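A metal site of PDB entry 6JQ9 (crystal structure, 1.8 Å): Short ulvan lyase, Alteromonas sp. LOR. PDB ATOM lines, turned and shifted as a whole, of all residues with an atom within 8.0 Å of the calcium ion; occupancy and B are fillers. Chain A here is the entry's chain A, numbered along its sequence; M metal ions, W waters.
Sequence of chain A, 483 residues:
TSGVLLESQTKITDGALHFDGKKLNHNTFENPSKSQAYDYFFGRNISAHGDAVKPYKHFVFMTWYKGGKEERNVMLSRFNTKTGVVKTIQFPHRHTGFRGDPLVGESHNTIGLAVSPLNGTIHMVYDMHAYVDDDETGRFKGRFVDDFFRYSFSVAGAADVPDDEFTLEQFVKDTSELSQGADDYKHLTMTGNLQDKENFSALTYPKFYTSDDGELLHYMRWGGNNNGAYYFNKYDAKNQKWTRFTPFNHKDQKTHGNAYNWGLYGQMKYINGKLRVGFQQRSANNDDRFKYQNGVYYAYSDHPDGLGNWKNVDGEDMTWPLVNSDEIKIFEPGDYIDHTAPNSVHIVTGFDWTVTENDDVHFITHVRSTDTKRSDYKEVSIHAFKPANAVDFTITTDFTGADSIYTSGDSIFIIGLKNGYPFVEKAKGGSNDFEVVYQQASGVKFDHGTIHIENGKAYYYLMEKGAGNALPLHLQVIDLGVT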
ATOM      1  N   ASN A 226     -18.533  -3.464  -0.223  1.00  0.00           N
ATOM      2  CA  ASN A 226     -18.954  -2.972  -1.555  1.00  0.00           C
ATOM      3  C   ASN A 226     -18.574  -1.506  -1.696  1.00  0.00           C
ATOM      4  O   ASN A 226     -19.211  -0.884  -2.518  1.00  0.00           O
ATOM      5  CB  ASN A 226     -20.442  -3.134  -1.872  1.00  0.00           C
ATOM      6  CG  ASN A 226     -21.328  -2.857  -0.685  1.00  0.00           C
ATOM      7  OD1 ASN A 226     -21.026  -1.949   0.087  1.00  0.00           O
ATOM      8  ND2 ASN A 226     -22.402  -3.634  -0.536  1.00  0.00           N
ATOM      9  N   GLN A 281     -14.301  -6.565  -8.912  1.00  0.00           N
ATOM     10  CA  GLN A 281     -15.020  -5.590  -8.053  1.00  0.00           C
ATOM     11  C   GLN A 281     -16.130  -6.272  -7.258  1.00  0.00           C
ATOM     12  O   GLN A 281     -16.589  -7.309  -7.683  1.00  0.00           O
ATOM     13  CB  GLN A 281     -15.737  -4.522  -8.889  1.00  0.00           C
ATOM     14  CG  GLN A 281     -17.022  -5.033  -9.517  1.00  0.00           C
ATOM     15  CD  GLN A 281     -17.833  -3.952 -10.174  1.00  0.00           C
ATOM     16  OE1 GLN A 281     -17.461  -2.804 -10.150  1.00  0.00           O
ATOM     17  NE2 GLN A 281     -18.891  -4.342 -10.844  1.00  0.00           N
ATOM     18  N   ARG A 282     -16.495  -5.669  -6.140  1.00  0.00           N
ATOM     19  CA  ARG A 282     -17.796  -6.068  -5.532  1.00  0.00           C
ATOM     20  C   ARG A 282     -18.739  -4.873  -5.522  1.00  0.00           C
ATOM     21  O   ARG A 282     -18.503  -3.978  -4.709  1.00  0.00           O
ATOM     22  CB  ARG A 282     -17.640  -6.565  -4.091  1.00  0.00           C
ATOM     23  CG  ARG A 282     -18.945  -6.985  -3.424  1.00  0.00           C
ATOM     24  CD  ARG A 282     -18.765  -7.297  -1.942  1.00  0.00           C
ATOM     25  NE  ARG A 282     -17.870  -8.431  -1.855  1.00  0.00           N
ATOM     26  CZ  ARG A 282     -17.494  -9.052  -0.747  1.00  0.00           C
ATOM     27  NH1 ARG A 282     -17.966  -8.686   0.433  1.00  0.00           N
ATOM     28  NH2 ARG A 282     -16.630 -10.047  -0.836  1.00  0.00           N
ATOM     29  N   SER A 283     -19.734  -4.896  -6.396  1.00  0.00           N
ATOM     30  CA  SER A 283     -20.788  -3.867  -6.546  1.00  0.00           C
ATOM     31  C   SER A 283     -21.684  -3.913  -5.313  1.00  0.00           C
ATOM     32  O   SER A 283     -21.955  -5.040  -4.804  1.00  0.00           O
ATOM     33  CB  SER A 283     -21.578  -4.097  -7.818  1.00  0.00           C
ATOM     34  OG  SER A 283     -22.694  -3.259  -7.865  1.00  0.00           O
ATOM     35  N   ALA A 284     -22.238  -2.773  -4.894  1.00  0.00           N
ATOM     36  CA  ALA A 284     -23.248  -2.740  -3.815  1.00  0.00           C
ATOM     37  C   ALA A 284     -24.604  -3.243  -4.324  1.00  0.00           C
ATOM     38  O   ALA A 284     -25.507  -3.327  -3.532  1.00  0.00           O
ATOM     39  CB  ALA A 284     -23.370  -1.336  -3.233  1.00  0.00           C
ATOM     40  N   ASN A 285     -24.747  -3.526  -5.620  1.00  0.00           N
ATOM     41  CA  ASN A 285     -26.007  -4.033  -6.203  1.00  0.00           C
ATOM     42  C   ASN A 285     -26.206  -5.459  -5.715  1.00  0.00           C
ATOM     43  O   ASN A 285     -25.352  -6.337  -6.044  1.00  0.00           O
ATOM     44  CB  ASN A 285     -26.019  -3.975  -7.716  1.00  0.00           C
ATOM     45  CG  ASN A 285     -27.261  -4.577  -8.354  1.00  0.00           C
ATOM     46  OD1 ASN A 285     -28.080  -5.207  -7.713  1.00  0.00           O
ATOM     47  ND2 ASN A 285     -27.385  -4.404  -9.661  1.00  0.00           N
ATOM     48  N   ASN A 286     -27.303  -5.694  -4.985  1.00  0.00           N
ATOM     49  CA  ASN A 286     -27.567  -7.023  -4.369  1.00  0.00           C
ATOM     50  C   ASN A 286     -28.750  -7.713  -5.074  1.00  0.00           C
ATOM     51  O   ASN A 286     -29.248  -8.737  -4.560  1.00  0.00           O
ATOM     52  CB  ASN A 286     -27.753  -6.910  -2.847  1.00  0.00           C
ATOM     53  CG  ASN A 286     -26.492  -6.587  -2.063  1.00  0.00           C
ATOM     54  OD1 ASN A 286     -25.361  -6.904  -2.478  1.00  0.00           O
ATOM     55  ND2 ASN A 286     -26.682  -6.005  -0.886  1.00  0.00           N
ATOM     56  N   ASP A 287     -29.133  -7.245  -6.258  1.00  0.00           N
ATOM     57  CA  ASP A 287     -30.248  -7.884  -7.009  1.00  0.00           C
ATOM     58  C   ASP A 287     -29.722  -8.552  -8.283  1.00  0.00           C
ATOM     59  O   ASP A 287     -30.457  -9.309  -8.861  1.00  0.00           O
ATOM     60  CB  ASP A 287     -31.355  -6.863  -7.322  1.00  0.00           C
ATOM     61  CG  ASP A 287     -31.993  -6.210  -6.102  1.00  0.00           C
ATOM     62  OD1 ASP A 287     -32.238  -6.916  -5.132  1.00  0.00           O
ATOM     63  OD2 ASP A 287     -32.228  -5.000  -6.141  1.00  0.00           O
ATOM     64  N   ASP A 288     -28.448  -8.337  -8.639  1.00  0.00           N
ATOM     65  CA  ASP A 288     -27.859  -8.991  -9.844  1.00  0.00           C
ATOM     66  C   ASP A 288     -27.401 -10.407  -9.509  1.00  0.00           C
ATOM     67  O   ASP A 288     -27.405 -10.746  -8.377  1.00  0.00           O
ATOM     68  CB  ASP A 288     -26.733  -8.163 -10.492  1.00  0.00           C
ATOM     69  CG  ASP A 288     -25.462  -8.014  -9.688  1.00  0.00           C
ATOM     70  OD1 ASP A 288     -24.566  -7.308 -10.184  1.00  0.00           O
ATOM     71  OD2 ASP A 288     -25.349  -8.620  -8.663  1.00  0.00           O
ATOM     72  N   ARG A 289     -26.987 -11.172 -10.523  1.00  0.00           N
ATOM     73  CA  ARG A 289     -26.567 -12.593 -10.408  1.00  0.00           C
ATOM     74  C   ARG A 289     -25.289 -12.818  -9.594  1.00  0.00           C
ATOM     75  O   ARG A 289     -25.099 -13.878  -9.157  1.00  0.00           O
ATOM     76  CB  ARG A 289     -26.466 -13.214 -11.801  1.00  0.00           C
ATOM     77  CG  ARG A 289     -25.557 -12.441 -12.733  1.00  0.00           C
ATOM     78  CD  ARG A 289     -25.730 -12.743 -14.223  1.00  0.00           C
ATOM     79  NE  ARG A 289     -25.358 -14.118 -14.455  1.00  0.00           N
ATOM     80  CZ  ARG A 289     -24.343 -14.494 -15.207  1.00  0.00           C
ATOM     81  NH1 ARG A 289     -24.082 -15.772 -15.347  1.00  0.00           N
ATOM     82  NH2 ARG A 289     -23.587 -13.582 -15.788  1.00  0.00           N
ATOM     83  N   PHE A 290     -24.463 -11.795  -9.385  1.00  0.00           N
ATOM     84  CA  PHE A 290     -23.188 -11.969  -8.652  1.00  0.00           C
ATOM     85  C   PHE A 290     -23.384 -11.728  -7.155  1.00  0.00           C
ATOM     86  O   PHE A 290     -23.572 -10.613  -6.802  1.00  0.00           O
ATOM     87  CB  PHE A 290     -22.154 -10.990  -9.194  1.00  0.00           C
ATOM     88  CG  PHE A 290     -21.976 -11.129 -10.664  1.00  0.00           C
ATOM     89  CD1 PHE A 290     -21.345 -12.241 -11.185  1.00  0.00           C
ATOM     90  CD2 PHE A 290     -22.497 -10.196 -11.536  1.00  0.00           C
ATOM     91  CE1 PHE A 290     -21.194 -12.377 -12.545  1.00  0.00           C
ATOM     92  CE2 PHE A 290     -22.352 -10.356 -12.894  1.00  0.00           C
ATOM     93  CZ  PHE A 290     -21.689 -11.436 -13.385  1.00  0.00           C
ATOM     94  N   LYS A 291     -23.238 -12.766  -6.339  1.00  0.00           N
ATOM     95  CA  LYS A 291     -23.448 -12.620  -4.866  1.00  0.00           C
ATOM     96  C   LYS A 291     -22.318 -11.752  -4.283  1.00  0.00           C
ATOM     97  O   LYS A 291     -22.630 -10.883  -3.417  1.00  0.00           O
ATOM     98  CB  LYS A 291     -23.590 -13.978  -4.171  1.00  0.00           C
ATOM     99  CG  LYS A 291     -23.845 -13.912  -2.676  1.00  0.00           C
ATOM    100  CD  LYS A 291     -23.820 -15.281  -2.005  1.00  0.00           C
ATOM    101  CE  LYS A 291     -24.855 -15.485  -0.908  1.00  0.00           C
ATOM    102  NZ  LYS A 291     -24.804 -16.863  -0.321  1.00  0.00           N
ATOM    103  N   TYR A 292     -21.100 -11.875  -4.816  1.00  0.00           N
ATOM    104  CA  TYR A 292     -19.908 -11.118  -4.327  1.00  0.00           C
ATOM    105  C   TYR A 292     -19.243 -10.383  -5.488  1.00  0.00           C
ATOM    106  O   TYR A 292     -19.848  -9.397  -5.972  1.00  0.00           O
ATOM    107  CB  TYR A 292     -18.977 -12.058  -3.553  1.00  0.00           C
ATOM    108  CG  TYR A 292     -19.643 -12.630  -2.327  1.00  0.00           C
ATOM    109  CD1 TYR A 292     -20.053 -11.799  -1.296  1.00  0.00           C
ATOM    110  CD2 TYR A 292     -19.885 -13.982  -2.200  1.00  0.00           C
ATOM    111  CE1 TYR A 292     -20.704 -12.292  -0.173  1.00  0.00           C
ATOM    112  CE2 TYR A 292     -20.480 -14.508  -1.057  1.00  0.00           C
ATOM    113  CZ  TYR A 292     -20.901 -13.650  -0.055  1.00  0.00           C
ATOM    114  OH  TYR A 292     -21.508 -14.149   1.058  1.00  0.00           O
ATOM    115  N   GLN A 293     -18.130 -10.896  -5.991  1.00  0.00           N
ATOM    116  CA  GLN A 293     -17.327 -10.217  -7.021  1.00  0.00           C
ATOM    117  C   GLN A 293     -17.911 -10.462  -8.422  1.00  0.00           C
ATOM    118  O   GLN A 293     -18.749 -11.366  -8.578  1.00  0.00           O
ATOM    119  CB  GLN A 293     -15.865 -10.625  -6.920  1.00  0.00           C
ATOM    120  CG  GLN A 293     -15.091  -9.847  -5.862  1.00  0.00           C
ATOM    121  CD  GLN A 293     -15.188 -10.392  -4.470  1.00  0.00           C
ATOM    122  OE1 GLN A 293     -16.118 -10.103  -3.726  1.00  0.00           O
ATOM    123  NE2 GLN A 293     -14.157 -11.120  -4.072  1.00  0.00           N
ATOM    124  N   ASN A 294     -17.502  -9.617  -9.371  1.00  0.00           N
ATOM    125  CA  ASN A 294     -17.710  -9.846 -10.813  1.00  0.00           C
ATOM    126  C   ASN A 294     -16.559  -9.175 -11.553  1.00  0.00           C
ATOM    127  O   ASN A 294     -15.901  -8.280 -10.932  1.00  0.00           O
ATOM    128  CB  ASN A 294     -19.077  -9.335 -11.215  1.00  0.00           C
ATOM    129  CG  ASN A 294     -19.120  -7.852 -11.475  1.00  0.00           C
ATOM    130  OD1 ASN A 294     -19.171  -7.061 -10.536  1.00  0.00           O
ATOM    131  ND2 ASN A 294     -19.011  -7.471 -12.743  1.00  0.00           N
ATOM    132  N   PRO A 342     -30.887 -13.849  -9.258  1.00  0.00           N
ATOM    133  CA  PRO A 342     -30.116 -13.008  -8.322  1.00  0.00           C
ATOM    134  C   PRO A 342     -29.201 -13.855  -7.421  1.00  0.00           C
ATOM    135  O   PRO A 342     -29.579 -14.898  -7.001  1.00  0.00           O
ATOM    136  CB  PRO A 342     -31.233 -12.286  -7.566  1.00  0.00           C
ATOM    137  CG  PRO A 342     -32.342 -12.184  -8.589  1.00  0.00           C
ATOM    138  CD  PRO A 342     -32.320 -13.527  -9.265  1.00  0.00           C
ATOM    139  N   ASN A 343     -27.960 -13.392  -7.259  1.00  0.00           N
ATOM    140  CA  ASN A 343     -26.961 -13.945  -6.310  1.00  0.00           C
ATOM    141  C   ASN A 343     -26.538 -15.391  -6.648  1.00  0.00           C
ATOM    142  O   ASN A 343     -25.958 -16.018  -5.770  1.00  0.00           O
ATOM    143  CB  ASN A 343     -27.535 -13.789  -4.900  1.00  0.00           C
ATOM    144  CG  ASN A 343     -27.584 -12.346  -4.484  1.00  0.00           C
ATOM    145  OD1 ASN A 343     -26.530 -11.712  -4.378  1.00  0.00           O
ATOM    146  ND2 ASN A 343     -28.762 -11.763  -4.364  1.00  0.00           N
ATOM    147  N   VAL A 345     -24.242 -16.562  -8.762  1.00  0.00           N
ATOM    148  CA  VAL A 345     -22.840 -16.713  -9.237  1.00  0.00           C
ATOM    149  C   VAL A 345     -21.904 -16.251  -8.130  1.00  0.00           C
ATOM    150  O   VAL A 345     -21.986 -15.092  -7.671  1.00  0.00           O
ATOM    151  CB  VAL A 345     -22.611 -15.964 -10.568  1.00  0.00           C
ATOM    152  CG1 VAL A 345     -21.165 -15.946 -10.970  1.00  0.00           C
ATOM    153  CG2 VAL A 345     -23.510 -16.490 -11.692  1.00  0.00           C
HETATM  154 CA    CA M   1     -24.220  -8.401  -6.525  1.00  0.00          CA
HETATM  155  O   HOH W   1     -24.906  -9.037  -4.168  1.00  0.00           O
HETATM  156  O   HOH W   2     -22.186  -8.032  -5.402  1.00  0.00           O
HETATM  157  O   HOH W   3     -22.886  -7.412  -8.132  1.00  0.00           O
HETATM  158  O   HOH W   4     -26.139  -9.670  -6.437  1.00  0.00           O
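The nearest printed residue that does not touch the calcium ion is Asn 286 (4.2 Å).
Water W4 lies within hydrogen-bond range of the backbone carbonyl oxygen of Asp 288 and the side-chain amide oxygen of Asn 343. Water W2 lies within hydrogen-bond range of O of Tyr 292 and O of Ser 283.
The calcium ion is bound by water W4 (2.3 Å), water W3 (2.3 Å), the backbone carbonyl oxygen (O) of Phe 290 (2.3 Å), water W2 (2.4 Å), the backbone carbonyl oxygen (O) of Asn 285 (2.4 Å), the side-chain carboxylate (OD2) of Asp 288 (2.4 Å) and water W1 (2.5 Å).
The backbone NH (N) of Asp 287 sits at hydrogen-bond distance from the side-chain amide oxygen (OD1) of Asn 285 (2.7 Å). N of Asn 285 lies within hydrogen-bond range of OG of Ser 283. O of Asp 288 lies within hydrogen-bond range of N of Asn 343, 2.9 Å away.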
